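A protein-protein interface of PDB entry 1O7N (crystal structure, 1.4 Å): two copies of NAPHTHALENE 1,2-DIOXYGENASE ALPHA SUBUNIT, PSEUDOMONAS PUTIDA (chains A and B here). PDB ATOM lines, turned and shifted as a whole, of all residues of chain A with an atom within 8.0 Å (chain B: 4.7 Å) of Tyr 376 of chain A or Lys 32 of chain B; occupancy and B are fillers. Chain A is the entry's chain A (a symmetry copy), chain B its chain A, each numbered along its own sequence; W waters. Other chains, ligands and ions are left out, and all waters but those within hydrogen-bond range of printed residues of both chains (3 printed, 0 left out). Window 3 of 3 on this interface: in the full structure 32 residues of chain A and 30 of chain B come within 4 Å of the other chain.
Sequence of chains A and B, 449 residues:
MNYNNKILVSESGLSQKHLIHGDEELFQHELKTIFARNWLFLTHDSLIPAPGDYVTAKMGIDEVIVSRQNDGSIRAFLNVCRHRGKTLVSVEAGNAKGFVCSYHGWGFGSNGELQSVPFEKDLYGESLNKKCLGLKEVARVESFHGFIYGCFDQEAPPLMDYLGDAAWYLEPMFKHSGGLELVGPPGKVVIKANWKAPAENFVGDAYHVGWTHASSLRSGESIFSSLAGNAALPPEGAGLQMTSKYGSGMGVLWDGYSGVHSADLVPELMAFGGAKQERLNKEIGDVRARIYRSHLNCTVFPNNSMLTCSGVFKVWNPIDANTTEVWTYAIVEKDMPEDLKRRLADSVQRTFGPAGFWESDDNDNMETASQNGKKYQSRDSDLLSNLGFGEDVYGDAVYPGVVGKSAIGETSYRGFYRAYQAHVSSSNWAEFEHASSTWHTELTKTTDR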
ATOM      1  N   GLN A 371      11.706 -16.497  -0.150  1.00  0.00           N
ATOM      2  CA  GLN A 371      11.155 -16.805   1.148  1.00  0.00           C
ATOM      3  C   GLN A 371       9.796 -17.505   1.062  1.00  0.00           C
ATOM      4  O   GLN A 371       9.455 -18.315   1.931  1.00  0.00           O
ATOM      5  CB  GLN A 371      11.068 -15.520   1.965  1.00  0.00           C
ATOM      6  CG  GLN A 371      12.469 -14.972   2.299  1.00  0.00           C
ATOM      7  CD  GLN A 371      12.468 -13.576   2.864  1.00  0.00           C
ATOM      8  OE1 GLN A 371      11.506 -13.172   3.538  1.00  0.00           O
ATOM      9  NE2 GLN A 371      13.527 -12.827   2.593  1.00  0.00           N
ATOM     10  N   ASN A 372       9.033 -17.186   0.007  1.00  0.00           N
ATOM     11  CA  ASN A 372       7.772 -17.868  -0.208  1.00  0.00           C
ATOM     12  C   ASN A 372       7.955 -19.356  -0.444  1.00  0.00           C
ATOM     13  O   ASN A 372       7.051 -20.119  -0.179  1.00  0.00           O
ATOM     14  CB  ASN A 372       6.985 -17.222  -1.348  1.00  0.00           C
ATOM     15  CG  ASN A 372       6.378 -15.904  -0.950  1.00  0.00           C
ATOM     16  OD1 ASN A 372       6.155 -15.648   0.266  1.00  0.00           O
ATOM     17  ND2 ASN A 372       6.107 -15.040  -1.918  1.00  0.00           N
ATOM     18  N   GLY A 373       9.136 -19.775  -0.932  1.00  0.00           N
ATOM     19  CA  GLY A 373       9.421 -21.192  -1.092  1.00  0.00           C
ATOM     20  C   GLY A 373       9.457 -21.988   0.193  1.00  0.00           C
ATOM     21  O   GLY A 373       9.445 -23.221   0.143  1.00  0.00           O
ATOM     22  N   LYS A 374       9.498 -21.292   1.349  1.00  0.00           N
ATOM     23  CA  LYS A 374       9.443 -21.976   2.648  1.00  0.00           C
ATOM     24  C   LYS A 374       8.013 -22.094   3.160  1.00  0.00           C
ATOM     25  O   LYS A 374       7.746 -22.900   4.068  1.00  0.00           O
ATOM     26  CB  LYS A 374      10.256 -21.232   3.720  1.00  0.00           C
ATOM     27  CG  LYS A 374      11.762 -21.307   3.500  1.00  0.00           C
ATOM     28  CD  LYS A 374      12.480 -20.648   4.678  1.00  0.00           C
ATOM     29  CE  LYS A 374      13.995 -20.766   4.503  1.00  0.00           C
ATOM     30  NZ  LYS A 374      14.423 -22.174   4.791  1.00  0.00           N
ATOM     31  N   LYS A 375       7.110 -21.300   2.606  1.00  0.00           N
ATOM     32  CA  LYS A 375       5.739 -21.280   3.149  1.00  0.00           C
ATOM     33  C   LYS A 375       4.977 -22.509   2.792  1.00  0.00           C
ATOM     34  O   LYS A 375       5.061 -22.985   1.655  1.00  0.00           O
ATOM     35  CB  LYS A 375       5.003 -20.045   2.664  1.00  0.00           C
ATOM     36  CG  LYS A 375       5.583 -18.766   3.278  1.00  0.00           C
ATOM     37  CD  LYS A 375       4.838 -17.535   2.800  1.00  0.00           C
ATOM     38  CE  LYS A 375       5.129 -16.306   3.639  1.00  0.00           C
ATOM     39  NZ  LYS A 375       6.465 -15.778   3.280  1.00  0.00           N
ATOM     40  N   TYR A 376       4.290 -23.082   3.771  1.00  0.00           N
ATOM     41  CA  TYR A 376       3.661 -24.392   3.604  1.00  0.00           C
ATOM     42  C   TYR A 376       2.808 -24.563   2.356  1.00  0.00           C
ATOM     43  O   TYR A 376       2.936 -25.584   1.638  1.00  0.00           O
ATOM     44  CB  TYR A 376       2.809 -24.670   4.853  1.00  0.00           C
ATOM     45  CG  TYR A 376       2.223 -26.061   4.817  1.00  0.00           C
ATOM     46  CD1 TYR A 376       2.954 -27.170   5.241  1.00  0.00           C
ATOM     47  CD2 TYR A 376       0.945 -26.271   4.333  1.00  0.00           C
ATOM     48  CE1 TYR A 376       2.417 -28.467   5.147  1.00  0.00           C
ATOM     49  CE2 TYR A 376       0.399 -27.535   4.261  1.00  0.00           C
ATOM     50  CZ  TYR A 376       1.128 -28.614   4.661  1.00  0.00           C
ATOM     51  OH  TYR A 376       0.580 -29.896   4.591  1.00  0.00           O
ATOM     52  N   GLN A 377       1.916 -23.606   2.090  1.00  0.00           N
ATOM     53  CA  GLN A 377       1.033 -23.768   0.931  1.00  0.00           C
ATOM     54  C   GLN A 377       1.698 -23.516  -0.413  1.00  0.00           C
ATOM     55  O   GLN A 377       1.092 -23.741  -1.467  1.00  0.00           O
ATOM     56  CB  GLN A 377      -0.219 -22.874   1.040  1.00  0.00           C
ATOM     57  CG  GLN A 377      -1.094 -23.243   2.227  1.00  0.00           C
ATOM     58  CD  GLN A 377      -1.881 -24.524   2.005  1.00  0.00           C
ATOM     59  OE1 GLN A 377      -2.133 -24.922   0.855  1.00  0.00           O
ATOM     60  NE2 GLN A 377      -2.214 -25.212   3.099  1.00  0.00           N
ATOM     61  N   SER A 378       2.940 -23.046  -0.399  1.00  0.00           N
ATOM     62  CA  SER A 378       3.672 -22.788  -1.657  1.00  0.00           C
ATOM     63  C   SER A 378       4.762 -23.793  -1.960  1.00  0.00           C
ATOM     64  O   SER A 378       5.226 -23.831  -3.115  1.00  0.00           O
ATOM     65  CB  SER A 378       4.280 -21.388  -1.628  1.00  0.00           C
ATOM     66  OG  SER A 378       3.287 -20.384  -1.667  1.00  0.00           O
ATOM     67  N   ARG A 379       5.203 -24.596  -0.994  1.00  0.00           N
ATOM     68  CA  ARG A 379       6.323 -25.487  -1.233  1.00  0.00           C
ATOM     69  C   ARG A 379       6.117 -26.351  -2.486  1.00  0.00           C
ATOM     70  O   ARG A 379       7.041 -26.522  -3.291  1.00  0.00           O
ATOM     71  CB  ARG A 379       6.546 -26.379  -0.028  1.00  0.00           C
ATOM     72  CG  ARG A 379       7.055 -25.631   1.210  1.00  0.00           C
ATOM     73  CD  ARG A 379       7.068 -26.499   2.437  1.00  0.00           C
ATOM     74  NE  ARG A 379       7.225 -25.670   3.643  1.00  0.00           N
ATOM     75  CZ  ARG A 379       7.083 -26.130   4.886  1.00  0.00           C
ATOM     76  NH1 ARG A 379       6.759 -27.397   5.129  1.00  0.00           N
ATOM     77  NH2 ARG A 379       7.271 -25.273   5.890  1.00  0.00           N
ATOM     78  N   ASP A 380       4.909 -26.885  -2.627  1.00  0.00           N
ATOM     79  CA  ASP A 380       4.611 -27.828  -3.717  1.00  0.00           C
ATOM     80  C   ASP A 380       3.943 -27.138  -4.890  1.00  0.00           C
ATOM     81  O   ASP A 380       3.390 -27.813  -5.786  1.00  0.00           O
ATOM     82  CB  ASP A 380       3.725 -28.964  -3.173  1.00  0.00           C
ATOM     83  CG  ASP A 380       3.334 -29.997  -4.231  1.00  0.00           C
ATOM     84  OD1 ASP A 380       4.218 -30.435  -5.017  1.00  0.00           O
ATOM     85  OD2 ASP A 380       2.150 -30.436  -4.310  1.00  0.00           O
ATOM     86  N   SER A 381       3.966 -25.815  -4.910  1.00  0.00           N
ATOM     87  CA  SER A 381       3.419 -25.068  -6.038  1.00  0.00           C
ATOM     88  C   SER A 381       4.423 -24.984  -7.163  1.00  0.00           C
ATOM     89  O   SER A 381       5.610 -25.196  -6.957  1.00  0.00           O
ATOM     90  CB  SER A 381       2.983 -23.661  -5.626  1.00  0.00           C
ATOM     91  OG  SER A 381       1.942 -23.792  -4.664  1.00  0.00           O
ATOM     92  N   GLN B  28       6.711 -28.123  12.342  1.00  0.00           N
ATOM     93  CA  GLN B  28       6.458 -28.351  10.918  1.00  0.00           C
ATOM     94  C   GLN B  28       5.248 -29.277  10.707  1.00  0.00           C
ATOM     95  O   GLN B  28       4.433 -29.078   9.789  1.00  0.00           O
ATOM     96  CB  GLN B  28       7.704 -28.937  10.248  1.00  0.00           C
ATOM     97  CG  GLN B  28       8.855 -27.921  10.173  1.00  0.00           C
ATOM     98  CD  GLN B  28       8.518 -26.707   9.345  1.00  0.00           C
ATOM     99  OE1 GLN B  28       8.025 -26.852   8.215  1.00  0.00           O
ATOM    100  NE2 GLN B  28       8.794 -25.506   9.872  1.00  0.00           N
ATOM    101  N   HIS B  29       5.124 -30.272  11.567  1.00  0.00           N
ATOM    102  CA  HIS B  29       4.005 -31.195  11.483  1.00  0.00           C
ATOM    103  C   HIS B  29       2.663 -30.496  11.819  1.00  0.00           C
ATOM    104  O   HIS B  29       1.617 -30.821  11.211  1.00  0.00           O
ATOM    105  CB  HIS B  29       4.267 -32.372  12.412  1.00  0.00           C
ATOM    106  CG  HIS B  29       3.214 -33.425  12.392  1.00  0.00           C
ATOM    107  ND1 HIS B  29       2.995 -34.229  11.288  1.00  0.00           N
ATOM    108  CD2 HIS B  29       2.329 -33.810  13.342  1.00  0.00           C
ATOM    109  CE1 HIS B  29       2.003 -35.064  11.574  1.00  0.00           C
ATOM    110  NE2 HIS B  29       1.589 -34.831  12.812  1.00  0.00           N
ATOM    111  N   GLU B  30       2.690 -29.537  12.751  1.00  0.00           N
ATOM    112  CA  GLU B  30       1.506 -28.731  13.055  1.00  0.00           C
ATOM    113  C   GLU B  30       1.075 -27.886  11.888  1.00  0.00           C
ATOM    114  O   GLU B  30      -0.105 -27.617  11.697  1.00  0.00           O
ATOM    115  CB  GLU B  30       1.734 -27.779  14.235  1.00  0.00           C
ATOM    116  CG  GLU B  30       1.910 -28.445  15.575  1.00  0.00           C
ATOM    117  CD  GLU B  30       2.344 -27.481  16.662  1.00  0.00           C
ATOM    118  OE1 GLU B  30       2.830 -26.374  16.311  1.00  0.00           O
ATOM    119  OE2 GLU B  30       2.277 -27.868  17.855  1.00  0.00           O
ATOM    120  N   LEU B  31       2.035 -27.453  11.069  1.00  0.00           N
ATOM    121  CA  LEU B  31       1.638 -26.663   9.896  1.00  0.00           C
ATOM    122  C   LEU B  31       0.648 -27.488   9.051  1.00  0.00           C
ATOM    123  O   LEU B  31      -0.329 -26.937   8.513  1.00  0.00           O
ATOM    124  CB  LEU B  31       2.855 -26.243   9.032  1.00  0.00           C
ATOM    125  CG  LEU B  31       3.840 -25.312   9.745  1.00  0.00           C
ATOM    126  CD1 LEU B  31       5.022 -25.054   8.806  1.00  0.00           C
ATOM    127  CD2 LEU B  31       3.169 -24.026  10.203  1.00  0.00           C
ATOM    128  N   LYS B  32       0.912 -28.792   8.927  1.00  0.00           N
ATOM    129  CA  LYS B  32       0.023 -29.670   8.172  1.00  0.00           C
ATOM    130  C   LYS B  32      -1.258 -30.055   8.908  1.00  0.00           C
ATOM    131  O   LYS B  32      -2.359 -29.971   8.357  1.00  0.00           O
ATOM    132  CB  LYS B  32       0.799 -30.919   7.783  1.00  0.00           C
ATOM    133  CG  LYS B  32      -0.101 -31.967   7.133  1.00  0.00           C
ATOM    134  CD  LYS B  32       0.662 -33.166   6.637  1.00  0.00           C
ATOM    135  CE  LYS B  32       1.700 -33.645   7.633  1.00  0.00           C
ATOM    136  NZ  LYS B  32       2.423 -34.844   7.032  1.00  0.00           N
ATOM    137  N   THR B  33      -1.119 -30.469  10.163  1.00  0.00           N
ATOM    138  CA  THR B  33      -2.230 -31.135  10.863  1.00  0.00           C
ATOM    139  C   THR B  33      -3.037 -30.195  11.742  1.00  0.00           C
ATOM    140  O   THR B  33      -4.165 -30.540  12.114  1.00  0.00           O
ATOM    141  CB  THR B  33      -1.720 -32.321  11.665  1.00  0.00           C
ATOM    142  OG1 THR B  33      -0.788 -31.881  12.671  1.00  0.00           O
ATOM    143  CG2 THR B  33      -0.868 -33.167  10.667  1.00  0.00           C
ATOM    144  N   ILE B  34      -2.512 -29.012  12.027  1.00  0.00           N
ATOM    145  CA  ILE B  34      -3.252 -28.016  12.789  1.00  0.00           C
ATOM    146  C   ILE B  34      -3.632 -26.879  11.856  1.00  0.00           C
ATOM    147  O   ILE B  34      -4.789 -26.577  11.634  1.00  0.00           O
ATOM    148  CB  ILE B  34      -2.412 -27.494  13.968  1.00  0.00           C
ATOM    149  CG1 ILE B  34      -2.106 -28.620  14.973  1.00  0.00           C
ATOM    150  CG2 ILE B  34      -3.166 -26.365  14.671  1.00  0.00           C
ATOM    151  CD1 ILE B  34      -3.346 -29.246  15.645  1.00  0.00           C
ATOM    152  N   ALA B  36      -3.106 -26.177   8.473  1.00  0.00           N
ATOM    153  CA  ALA B  36      -3.698 -26.404   7.150  1.00  0.00           C
ATOM    154  C   ALA B  36      -5.072 -27.080   7.233  1.00  0.00           C
ATOM    155  O   ALA B  36      -5.778 -27.141   6.222  1.00  0.00           O
ATOM    156  CB  ALA B  36      -2.751 -27.238   6.260  1.00  0.00           C
ATOM    157  N   ARG B  37      -5.474 -27.501   8.418  1.00  0.00           N
ATOM    158  CA  ARG B  37      -6.689 -28.299   8.606  1.00  0.00           C
ATOM    159  C   ARG B  37      -7.845 -27.563   9.258  1.00  0.00           C
ATOM    160  O   ARG B  37      -9.012 -27.879   9.025  1.00  0.00           O
ATOM    161  CB  ARG B  37      -6.365 -29.511   9.494  1.00  0.00           C
ATOM    162  CG  ARG B  37      -7.559 -30.560   9.542  1.00  0.00           C
ATOM    163  CD  ARG B  37      -7.239 -31.965  10.120  1.00  0.00           C
ATOM    164  NE  ARG B  37      -6.101 -32.623   9.492  1.00  0.00           N
ATOM    165  CZ  ARG B  37      -5.231 -33.402  10.100  1.00  0.00           C
ATOM    166  NH1 ARG B  37      -5.371 -33.612  11.441  1.00  0.00           N
ATOM    167  NH2 ARG B  37      -4.194 -33.920   9.495  1.00  0.00           N
ATOM    168  N   ILE B  61       1.869 -20.103   8.705  1.00  0.00           N
ATOM    169  CA  ILE B  61       2.985 -19.289   8.203  1.00  0.00           C
ATOM    170  C   ILE B  61       2.715 -18.709   6.820  1.00  0.00           C
ATOM    171  O   ILE B  61       3.509 -17.901   6.310  1.00  0.00           O
ATOM    172  CB  ILE B  61       4.343 -20.043   8.203  1.00  0.00           C
ATOM    173  CG1 ILE B  61       4.345 -21.213   7.187  1.00  0.00           C
ATOM    174  CG2 ILE B  61       4.710 -20.454   9.645  1.00  0.00           C
ATOM    175  CD1 ILE B  61       5.757 -21.820   7.003  1.00  0.00           C
ATOM    176  N   ASP B  62       1.597 -19.080   6.209  1.00  0.00           N
ATOM    177  CA  ASP B  62       1.249 -18.511   4.909  1.00  0.00           C
ATOM    178  C   ASP B  62       0.603 -17.155   5.062  1.00  0.00           C
ATOM    179  O   ASP B  62       0.055 -16.838   6.120  1.00  0.00           O
ATOM    180  CB  ASP B  62       0.293 -19.457   4.171  1.00  0.00           C
ATOM    181  CG  ASP B  62       0.900 -20.796   3.954  1.00  0.00           C
ATOM    182  OD1 ASP B  62       1.691 -20.901   2.973  1.00  0.00           O
ATOM    183  OD2 ASP B  62       0.672 -21.784   4.699  1.00  0.00           O
HETATM  184  O   HOH W   1       5.532 -29.048   7.212  1.00  0.00           O
HETATM  185  O   HOH W   2       9.171 -29.121   6.858  1.00  0.00           O
HETATM  186  O   HOH W   3       2.199 -19.461   0.718  1.00  0.00           O
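OE1 of Gln 28 of chain B is in hydrogen-bond range of NH2 of Arg 379 of chain A, at 2.9 Å. N of Tyr 376 of chain A lies within hydrogen-bond range of OD1 of Asp 62 of chain B (3.5 Å). The backbone NH (N) of Gln 377 of chain A lies within hydrogen-bond range of the side-chain carboxylate (OD1) of Asp 62 of chain B, at 2.9 Å.
The backbone carbonyl oxygen (O) of Leu 31 of chain B is in hydrogen-bond range of the backbone NH (N) of Ala 36 of chain B (2.9 Å). OD1 of Asn 372 of chain A is in hydrogen-bond range of NZ of Lys 375 of chain A (3.0 Å). The guanidinium group of Arg 379 of chain A is in hydrogen-bond range of the backbone carbonyl oxygen of Lys 374 of chain A, 2.9 Å away. O of Gln 377 of chain A sits at hydrogen-bond distance from OG of Ser 381 of chain A (3.3 Å).
Lys 374 of chain A touches Ile 61 of chain B (O to CD1, 3.7 Å). CE of Lys 375 of chain A touches O of Ile 61 of chain B, at 3.5 Å. Asp 62 of chain B touches Lys 375 of chain A. Leu 31 of chain B touches Tyr 376 of chain A. OH of Tyr 376 of chain A touches CG of Lys 32 of chain B (3.3 Å). Tyr 376 of chain A touches Ala 36 of chain B. Tyr 376 of chain A touches Ile 61 of chain B (N to CD1, 3.8 Å). Gln 377 of chain A touches Ala 36 of chain B. NH2 of Arg 379 of chain A touches CD1 of Leu 31 of chain B, at 3.7 Å. Ile 61 of chain B touches Arg 379 of chain A (CD1 to NH2, 3.9 Å).
Tyr 376 of chain A touches just these residues of chain B: Leu 31, Lys 32, Ala 36, Ile 61 and Asp 62. Of chain A, only Tyr 376 comes within 4 Å of Lys 32 of chain B. Of the printed residues of chain A, Leu 31 of chain B touches Tyr 376 and Arg 379. Of the printed residues of chain B, Gln 377 of chain A touches Ala 36 (3.8 Å) and Asp 62 (2.9 Å). Of the printed residues of chain A, Gln 28 of chain B touches Arg 379 (2.9 Å). Of the printed residues of chain A, Ala 36 of chain B touches Tyr 376 and Gln 377. Of the printed residues of chain B, Lys 375 of chain A touches Ile 61 and Asp 62. His 29 of chain B touches none of the printed residues of chain A. The nearest printed residue of chain B that does not touch Tyr 376 of chain A is Gln 28 of chain B (5.1 Å). The nearest printed residue of chain A that does not touch Lys 32 of chain B is Gln 377 of chain A (7.1 Å).
Of the 11 printed residues of chain A, 5 touch a printed residue of chain B. Among the printed residues, no Asp or Glu carboxylate lies within 4 Å of a Lys or Arg side-chain nitrogen of the other chain.
No position is printed for both chains. Of the 13 pairs that touch across the chains among the printed residues, none has its exchanged pair printed and touching as well.
Water W3 bridges the side-chain carboxylate (OD1) of Asp 62 of chain B (2.7 Å) and the side-chain hydroxyl (OG) of Ser 378 of chain A (2.8 Å). Water W1 lies within hydrogen-bond range of O of Gln 28 of chain B (2.8 Å) and NH1 of Arg 379 of chain A (2.9 Å). Water W2 lies within hydrogen-bond range of OE1 of Gln 28 of chain B (2.9 Å) and NH1 of Arg 379 of chain A (3.4 Å).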
